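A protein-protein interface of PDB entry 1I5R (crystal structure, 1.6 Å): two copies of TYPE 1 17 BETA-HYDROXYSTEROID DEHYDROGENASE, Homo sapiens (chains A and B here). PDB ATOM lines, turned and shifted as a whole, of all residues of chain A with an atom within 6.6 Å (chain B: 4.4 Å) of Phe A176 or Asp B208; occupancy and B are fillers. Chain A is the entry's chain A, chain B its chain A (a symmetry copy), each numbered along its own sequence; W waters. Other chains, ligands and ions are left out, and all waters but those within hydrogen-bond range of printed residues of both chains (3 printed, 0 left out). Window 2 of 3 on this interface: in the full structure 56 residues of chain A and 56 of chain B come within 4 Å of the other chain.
NZ of Lys A130 lies within hydrogen-bond range of OG1 of Thr B211. The side-chain carboxylate (OD1) of Asp B208 is in salt-bridge range of the side-chain amino group (NZ) of Lys A130 (3.9 Å). NZ of Lys A130 is in salt-bridge range of OE2 of Glu B100, 2.7 Å away.
The side-chain hydroxyl (OG1) of Thr B207 is in hydrogen-bond range of the side-chain carboxylate (OD1) of Asp B208, at 3.5 Å. N of His B210 lies within hydrogen-bond range of OD2 of Asp B208 (3.0 Å). The side-chain hydroxyl (OG1) of Thr B211 lies within hydrogen-bond range of the side-chain carboxylate (OD1) of Asp B208. OE2 of Glu B100 is in hydrogen-bond range of OG1 of Thr B207, at 2.7 Å.
Among the printed residues, merely in contact across the chains: Pro A127 with Glu B100 (3.8 Å), Leu A172 with Arg B214 (3.6 Å), Pro A175 with Arg B214 (3.7 Å), Phe A176 with Asp B208 (3.9 Å) and Phe A176 with Thr B211 (3.3 Å).
Of the printed residues of chain B, Pro A127 touches Glu B100. Of the printed residues of chain B, Lys A130 touches Glu B100 (2.7 Å), Asp B208 (3.8 Å) and Thr B211 (2.7 Å). Printed residues of chain B within 4 Å of Pro A175: Arg B214 (3.7 Å). Of the printed residues of chain B, Phe A176 touches Asp B208 (3.9 Å) and Thr B211 (3.3 Å). Printed residues of chain A within 4 Å of Glu B100: Pro A127 and Lys A130. Of chain A, only Lys A130 (3.8 Å) and Phe A176 (3.9 Å) come within 4 Å of Asp B208. Of the printed residues of chain A, Arg B214 touches Leu A172 (3.6 Å) and Pro A175 (3.7 Å). The nearest printed residue of chain B that does not touch Phe A176 is His B210 (4.01 Å). The nearest printed residue of chain A that does not touch Thr B211 is Leu A172 (4.1 Å).
Of the 16 printed residues of chain A, 5 touch a printed residue of chain B. Printed residues of chain A that touch a printed residue of chain B: Pro A127, Lys A130, Leu A172, Pro A175 and Phe A176. Of the 8 printed residues of chain B, 4 touch a printed residue of chain A. Among the printed residues, 8 pairs touch across the chains. Among the printed residues, Asp or Glu carboxylates within 4 Å of a Lys or Arg side-chain nitrogen of the other chain: Lys A130 with Glu B100 (2.7 Å) and Lys A130 with Asp B208 (3.9 Å).
No position is printed for both chains. Of the 8 pairs that touch across the chains among the printed residues, none has its exchanged pair printed and touching as well.
Water W3 lies within hydrogen-bond range of NZ of Lys A130 (2.7 Å) and OE1 of Glu B100 (2.8 Å). Water W1 lies within hydrogen-bond range of the side-chain carboxylate of Asp B208 and the backbone carbonyl oxygen of Lys A130. Water W2 bridges O of Leu A172 (2.8 Å) and NE of Arg B214 (3.1 Å).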
ATOM      1  N   PRO A 127     -22.134 -26.373   9.503  1.00  0.00           N
ATOM      2  CA  PRO A 127     -22.177 -25.236   8.582  1.00  0.00           C
ATOM      3  C   PRO A 127     -22.119 -25.658   7.125  1.00  0.00           C
ATOM      4  O   PRO A 127     -22.960 -25.221   6.335  1.00  0.00           O
ATOM      5  CB  PRO A 127     -20.979 -24.390   8.980  1.00  0.00           C
ATOM      6  CG  PRO A 127     -20.867 -24.641  10.452  1.00  0.00           C
ATOM      7  CD  PRO A 127     -21.198 -26.114  10.616  1.00  0.00           C
ATOM      8  N   MET A 129     -22.837 -28.560   5.864  1.00  0.00           N
ATOM      9  CA  MET A 129     -24.051 -29.294   5.530  1.00  0.00           C
ATOM     10  C   MET A 129     -25.203 -28.342   5.273  1.00  0.00           C
ATOM     11  O   MET A 129     -25.957 -28.526   4.324  1.00  0.00           O
ATOM     12  CB  MET A 129     -24.421 -30.242   6.659  1.00  0.00           C
ATOM     13  CG  MET A 129     -23.248 -31.201   6.881  1.00  0.00           C
ATOM     14  SD  MET A 129     -23.847 -32.453   8.035  1.00  0.00           S
ATOM     15  CE  MET A 129     -22.547 -33.665   7.846  1.00  0.00           C
ATOM     16  N   LYS A 130     -25.369 -27.375   6.173  1.00  0.00           N
ATOM     17  CA  LYS A 130     -26.430 -26.392   5.992  1.00  0.00           C
ATOM     18  C   LYS A 130     -26.233 -25.654   4.670  1.00  0.00           C
ATOM     19  O   LYS A 130     -27.227 -25.413   3.993  1.00  0.00           O
ATOM     20  CB  LYS A 130     -26.406 -25.387   7.131  1.00  0.00           C
ATOM     21  CG  LYS A 130     -26.839 -25.980   8.465  1.00  0.00           C
ATOM     22  CD  LYS A 130     -26.565 -24.865   9.484  1.00  0.00           C
ATOM     23  CE  LYS A 130     -27.515 -24.894  10.652  1.00  0.00           C
ATOM     24  NZ  LYS A 130     -27.333 -23.618  11.406  1.00  0.00           N
ATOM     25  N   ARG A 131     -24.987 -25.322   4.363  1.00  0.00           N
ATOM     26  CA  ARG A 131     -24.664 -24.620   3.123  1.00  0.00           C
ATOM     27  C   ARG A 131     -25.037 -25.464   1.912  1.00  0.00           C
ATOM     28  O   ARG A 131     -25.636 -24.962   0.963  1.00  0.00           O
ATOM     29  CB  ARG A 131     -23.174 -24.279   3.071  1.00  0.00           C
ATOM     30  CG  ARG A 131     -22.782 -23.487   1.830  1.00  0.00           C
ATOM     31  CD  ARG A 131     -21.278 -23.321   1.722  1.00  0.00           C
ATOM     32  NE  ARG A 131     -20.576 -24.568   1.469  1.00  0.00           N
ATOM     33  CZ  ARG A 131     -20.669 -25.321   0.380  1.00  0.00           C
ATOM     34  NH1 ARG A 131     -21.463 -24.984  -0.630  1.00  0.00           N
ATOM     35  NH2 ARG A 131     -19.957 -26.437   0.290  1.00  0.00           N
ATOM     36  N   ARG A 132     -24.716 -26.749   1.954  1.00  0.00           N
ATOM     37  CA  ARG A 132     -25.024 -27.669   0.869  1.00  0.00           C
ATOM     38  C   ARG A 132     -26.505 -28.007   0.822  1.00  0.00           C
ATOM     39  O   ARG A 132     -27.044 -28.490  -0.177  1.00  0.00           O
ATOM     40  CB  ARG A 132     -24.233 -28.965   1.071  1.00  0.00           C
ATOM     41  CG  ARG A 132     -22.729 -28.797   0.983  1.00  0.00           C
ATOM     42  CD  ARG A 132     -22.042 -30.115   0.712  1.00  0.00           C
ATOM     43  NE  ARG A 132     -22.491 -31.264   1.473  1.00  0.00           N
ATOM     44  CZ  ARG A 132     -22.451 -31.434   2.783  1.00  0.00           C
ATOM     45  NH1 ARG A 132     -21.980 -30.442   3.517  1.00  0.00           N
ATOM     46  NH2 ARG A 132     -22.854 -32.527   3.418  1.00  0.00           N
ATOM     47  N   GLY A 133     -27.165 -27.909   1.977  1.00  0.00           N
ATOM     48  CA  GLY A 133     -28.569 -28.273   2.102  1.00  0.00           C
ATOM     49  C   GLY A 133     -28.656 -29.799   2.133  1.00  0.00           C
ATOM     50  O   GLY A 133     -29.654 -30.410   1.774  1.00  0.00           O
ATOM     51  N   SER A 134     -27.574 -30.418   2.615  1.00  0.00           N
ATOM     52  CA  SER A 134     -27.559 -31.873   2.686  1.00  0.00           C
ATOM     53  C   SER A 134     -26.516 -32.318   3.700  1.00  0.00           C
ATOM     54  O   SER A 134     -25.512 -31.659   3.964  1.00  0.00           O
ATOM     55  CB  SER A 134     -27.246 -32.499   1.324  1.00  0.00           C
ATOM     56  OG  SER A 134     -25.879 -32.328   1.005  1.00  0.00           O
ATOM     57  N   GLY A 135     -26.790 -33.496   4.248  1.00  0.00           N
ATOM     58  CA  GLY A 135     -25.839 -34.045   5.218  1.00  0.00           C
ATOM     59  C   GLY A 135     -26.664 -34.784   6.266  1.00  0.00           C
ATOM     60  O   GLY A 135     -27.779 -34.412   6.588  1.00  0.00           O
ATOM     61  N   LEU A 172     -34.359 -27.026  14.409  1.00  0.00           N
ATOM     62  CA  LEU A 172     -33.860 -26.011  13.497  1.00  0.00           C
ATOM     63  C   LEU A 172     -33.549 -26.587  12.127  1.00  0.00           C
ATOM     64  O   LEU A 172     -33.907 -26.010  11.102  1.00  0.00           O
ATOM     65  CB  LEU A 172     -32.572 -25.404  14.062  1.00  0.00           C
ATOM     66  CG  LEU A 172     -31.849 -24.468  13.091  1.00  0.00           C
ATOM     67  CD1 LEU A 172     -32.759 -23.295  12.729  1.00  0.00           C
ATOM     68  CD2 LEU A 172     -30.549 -23.993  13.698  1.00  0.00           C
ATOM     69  N   LEU A 173     -32.834 -27.719  12.117  1.00  0.00           N
ATOM     70  CA  LEU A 173     -32.344 -28.283  10.876  1.00  0.00           C
ATOM     71  C   LEU A 173     -33.373 -28.864   9.930  1.00  0.00           C
ATOM     72  O   LEU A 173     -33.058 -29.028   8.753  1.00  0.00           O
ATOM     73  CB  LEU A 173     -31.304 -29.375  11.175  1.00  0.00           C
ATOM     74  CG  LEU A 173     -30.029 -28.886  11.872  1.00  0.00           C
ATOM     75  CD1 LEU A 173     -29.185 -30.088  12.275  1.00  0.00           C
ATOM     76  CD2 LEU A 173     -29.268 -27.931  10.965  1.00  0.00           C
ATOM     77  N   LEU A 174     -34.593 -29.042  10.373  1.00  0.00           N
ATOM     78  CA  LEU A 174     -35.677 -29.617   9.612  1.00  0.00           C
ATOM     79  C   LEU A 174     -35.726 -29.127   8.178  1.00  0.00           C
ATOM     80  O   LEU A 174     -35.587 -29.942   7.263  1.00  0.00           O
ATOM     81  CB  LEU A 174     -37.004 -29.445  10.347  1.00  0.00           C
ATOM     82  CG  LEU A 174     -38.220 -30.160   9.753  1.00  0.00           C
ATOM     83  CD1 LEU A 174     -37.944 -31.639   9.501  1.00  0.00           C
ATOM     84  CD2 LEU A 174     -39.426 -30.021  10.675  1.00  0.00           C
ATOM     85  N   PRO A 175     -35.827 -27.831   7.936  1.00  0.00           N
ATOM     86  CA  PRO A 175     -35.897 -27.294   6.589  1.00  0.00           C
ATOM     87  C   PRO A 175     -34.572 -27.107   5.889  1.00  0.00           C
ATOM     88  O   PRO A 175     -34.543 -26.755   4.707  1.00  0.00           O
ATOM     89  CB  PRO A 175     -36.570 -25.935   6.796  1.00  0.00           C
ATOM     90  CG  PRO A 175     -36.025 -25.499   8.118  1.00  0.00           C
ATOM     91  CD  PRO A 175     -35.998 -26.766   8.948  1.00  0.00           C
ATOM     92  N   PHE A 176     -33.448 -27.383   6.545  1.00  0.00           N
ATOM     93  CA  PHE A 176     -32.141 -27.207   5.937  1.00  0.00           C
ATOM     94  C   PHE A 176     -31.733 -28.380   5.063  1.00  0.00           C
ATOM     95  O   PHE A 176     -30.717 -28.293   4.377  1.00  0.00           O
ATOM     96  CB  PHE A 176     -31.090 -27.023   7.040  1.00  0.00           C
ATOM     97  CG  PHE A 176     -31.091 -25.635   7.616  1.00  0.00           C
ATOM     98  CD1 PHE A 176     -32.010 -25.311   8.596  1.00  0.00           C
ATOM     99  CD2 PHE A 176     -30.185 -24.681   7.184  1.00  0.00           C
ATOM    100  CE1 PHE A 176     -32.041 -24.045   9.148  1.00  0.00           C
ATOM    101  CE2 PHE A 176     -30.207 -23.412   7.743  1.00  0.00           C
ATOM    102  CZ  PHE A 176     -31.129 -23.102   8.718  1.00  0.00           C
ATOM    103  N   GLY A 177     -32.424 -29.509   5.175  1.00  0.00           N
ATOM    104  CA  GLY A 177     -32.063 -30.693   4.401  1.00  0.00           C
ATOM    105  C   GLY A 177     -30.945 -31.460   5.107  1.00  0.00           C
ATOM    106  O   GLY A 177     -30.370 -32.399   4.565  1.00  0.00           O
ATOM    107  N   VAL A 178     -30.634 -31.045   6.329  1.00  0.00           N
ATOM    108  CA  VAL A 178     -29.583 -31.668   7.124  1.00  0.00           C
ATOM    109  C   VAL A 178     -30.318 -32.502   8.155  1.00  0.00           C
ATOM    110  O   VAL A 178     -31.155 -31.999   8.886  1.00  0.00           O
ATOM    111  CB  VAL A 178     -28.659 -30.650   7.795  1.00  0.00           C
ATOM    112  CG1 VAL A 178     -27.600 -31.354   8.621  1.00  0.00           C
ATOM    113  CG2 VAL A 178     -28.021 -29.813   6.694  1.00  0.00           C
ATOM    114  N   HIS A 179     -30.024 -33.793   8.144  1.00  0.00           N
ATOM    115  CA  HIS A 179     -30.770 -34.720   8.979  1.00  0.00           C
ATOM    116  C   HIS A 179     -29.924 -35.162  10.157  1.00  0.00           C
ATOM    117  O   HIS A 179     -28.838 -35.672   9.962  1.00  0.00           O
ATOM    118  CB  HIS A 179     -31.166 -35.932   8.133  1.00  0.00           C
ATOM    119  CG  HIS A 179     -31.935 -35.519   6.913  1.00  0.00           C
ATOM    120  ND1 HIS A 179     -33.212 -35.020   6.978  1.00  0.00           N
ATOM    121  CD2 HIS A 179     -31.576 -35.503   5.610  1.00  0.00           C
ATOM    122  CE1 HIS A 179     -33.628 -34.727   5.755  1.00  0.00           C
ATOM    123  NE2 HIS A 179     -32.652 -35.011   4.915  1.00  0.00           N
ATOM    124  N   GLU B 100     -23.225 -23.135  15.801  1.00  0.00           N
ATOM    125  CA  GLU B 100     -21.950 -22.761  15.221  1.00  0.00           C
ATOM    126  C   GLU B 100     -21.500 -21.355  15.583  1.00  0.00           C
ATOM    127  O   GLU B 100     -20.320 -21.015  15.435  1.00  0.00           O
ATOM    128  CB  GLU B 100     -21.983 -22.919  13.698  1.00  0.00           C
ATOM    129  CG  GLU B 100     -22.991 -22.000  13.031  1.00  0.00           C
ATOM    130  CD  GLU B 100     -24.347 -22.654  12.873  1.00  0.00           C
ATOM    131  OE1 GLU B 100     -24.735 -23.501  13.701  1.00  0.00           O
ATOM    132  OE2 GLU B 100     -25.043 -22.312  11.894  1.00  0.00           O
ATOM    133  N   THR B 207     -22.667 -17.426  11.519  1.00  0.00           N
ATOM    134  CA  THR B 207     -23.624 -18.403  11.003  1.00  0.00           C
ATOM    135  C   THR B 207     -24.069 -17.972   9.613  1.00  0.00           C
ATOM    136  O   THR B 207     -23.667 -16.903   9.157  1.00  0.00           O
ATOM    137  CB  THR B 207     -24.827 -18.592  11.941  1.00  0.00           C
ATOM    138  OG1 THR B 207     -25.593 -19.727  11.513  1.00  0.00           O
ATOM    139  CG2 THR B 207     -25.730 -17.368  11.911  1.00  0.00           C
ATOM    140  N   ASP B 208     -24.926 -18.771   9.007  1.00  0.00           N
ATOM    141  CA  ASP B 208     -25.422 -18.417   7.672  1.00  0.00           C
ATOM    142  C   ASP B 208     -26.661 -17.555   7.829  1.00  0.00           C
ATOM    143  O   ASP B 208     -27.329 -17.554   8.872  1.00  0.00           O
ATOM    144  CB  ASP B 208     -25.705 -19.685   6.880  1.00  0.00           C
ATOM    145  CG  ASP B 208     -26.823 -20.476   7.541  1.00  0.00           C
ATOM    146  OD1 ASP B 208     -26.520 -21.220   8.499  1.00  0.00           O
ATOM    147  OD2 ASP B 208     -27.972 -20.307   7.092  1.00  0.00           O
ATOM    148  N   ILE B 209     -27.031 -16.841   6.778  1.00  0.00           N
ATOM    149  CA  ILE B 209     -28.155 -15.914   6.795  1.00  0.00           C
ATOM    150  C   ILE B 209     -29.470 -16.638   7.060  1.00  0.00           C
ATOM    151  O   ILE B 209     -30.388 -16.042   7.646  1.00  0.00           O
ATOM    152  CB  ILE B 209     -28.274 -15.137   5.471  1.00  0.00           C
ATOM    153  CG1 ILE B 209     -29.313 -14.020   5.600  1.00  0.00           C
ATOM    154  CG2 ILE B 209     -28.630 -16.078   4.331  1.00  0.00           C
ATOM    155  CD1 ILE B 209     -29.333 -13.066   4.425  1.00  0.00           C
ATOM    156  N   HIS B 210     -29.628 -17.881   6.637  1.00  0.00           N
ATOM    157  CA  HIS B 210     -30.861 -18.625   6.837  1.00  0.00           C
ATOM    158  C   HIS B 210     -31.007 -19.004   8.312  1.00  0.00           C
ATOM    159  O   HIS B 210     -32.058 -18.828   8.912  1.00  0.00           O
ATOM    160  CB  HIS B 210     -30.906 -19.880   5.967  1.00  0.00           C
ATOM    161  CG  HIS B 210     -30.606 -19.518   4.536  1.00  0.00           C
ATOM    162  ND1 HIS B 210     -31.433 -18.670   3.825  1.00  0.00           N
ATOM    163  CD2 HIS B 210     -29.590 -19.860   3.714  1.00  0.00           C
ATOM    164  CE1 HIS B 210     -30.933 -18.513   2.611  1.00  0.00           C
ATOM    165  NE2 HIS B 210     -29.822 -19.218   2.523  1.00  0.00           N
ATOM    166  N   THR B 211     -29.896 -19.497   8.865  1.00  0.00           N
ATOM    167  CA  THR B 211     -29.919 -19.817  10.294  1.00  0.00           C
ATOM    168  C   THR B 211     -30.184 -18.547  11.094  1.00  0.00           C
ATOM    169  O   THR B 211     -30.953 -18.545  12.043  1.00  0.00           O
ATOM    170  CB  THR B 211     -28.580 -20.419  10.752  1.00  0.00           C
ATOM    171  OG1 THR B 211     -28.426 -21.634  10.025  1.00  0.00           O
ATOM    172  CG2 THR B 211     -28.626 -20.672  12.250  1.00  0.00           C
ATOM    173  N   PHE B 212     -29.528 -17.469  10.680  1.00  0.00           N
ATOM    174  CA  PHE B 212     -29.695 -16.188  11.358  1.00  0.00           C
ATOM    175  C   PHE B 212     -31.149 -15.750  11.308  1.00  0.00           C
ATOM    176  O   PHE B 212     -31.735 -15.333  12.305  1.00  0.00           O
ATOM    177  CB  PHE B 212     -28.774 -15.140  10.728  1.00  0.00           C
ATOM    178  CG  PHE B 212     -28.851 -13.841  11.485  1.00  0.00           C
ATOM    179  CD1 PHE B 212     -28.154 -13.701  12.675  1.00  0.00           C
ATOM    180  CD2 PHE B 212     -29.628 -12.795  11.023  1.00  0.00           C
ATOM    181  CE1 PHE B 212     -28.221 -12.514  13.388  1.00  0.00           C
ATOM    182  CE2 PHE B 212     -29.693 -11.614  11.733  1.00  0.00           C
ATOM    183  CZ  PHE B 212     -28.988 -11.477  12.910  1.00  0.00           C
ATOM    184  N   ARG B 214     -33.706 -17.746  10.955  1.00  0.00           N
ATOM    185  CA  ARG B 214     -34.457 -18.618  11.850  1.00  0.00           C
ATOM    186  C   ARG B 214     -34.242 -18.173  13.288  1.00  0.00           C
ATOM    187  O   ARG B 214     -35.120 -18.342  14.125  1.00  0.00           O
ATOM    188  CB  ARG B 214     -33.980 -20.061  11.687  1.00  0.00           C
ATOM    189  CG  ARG B 214     -34.329 -20.623  10.316  1.00  0.00           C
ATOM    190  CD  ARG B 214     -35.825 -20.681  10.120  1.00  0.00           C
ATOM    191  NE  ARG B 214     -36.180 -21.420   8.907  1.00  0.00           N
ATOM    192  CZ  ARG B 214     -37.438 -21.525   8.489  1.00  0.00           C
ATOM    193  NH1 ARG B 214     -38.414 -20.939   9.168  1.00  0.00           N
ATOM    194  NH2 ARG B 214     -37.685 -22.221   7.388  1.00  0.00           N
HETATM  195  O   HOH W   1     -27.856 -22.379   5.277  1.00  0.00           O
HETATM  196  O   HOH W   2     -35.710 -23.936  10.740  1.00  0.00           O
HETATM  197  O   HOH W   3     -27.379 -24.525  13.900  1.00  0.00           O
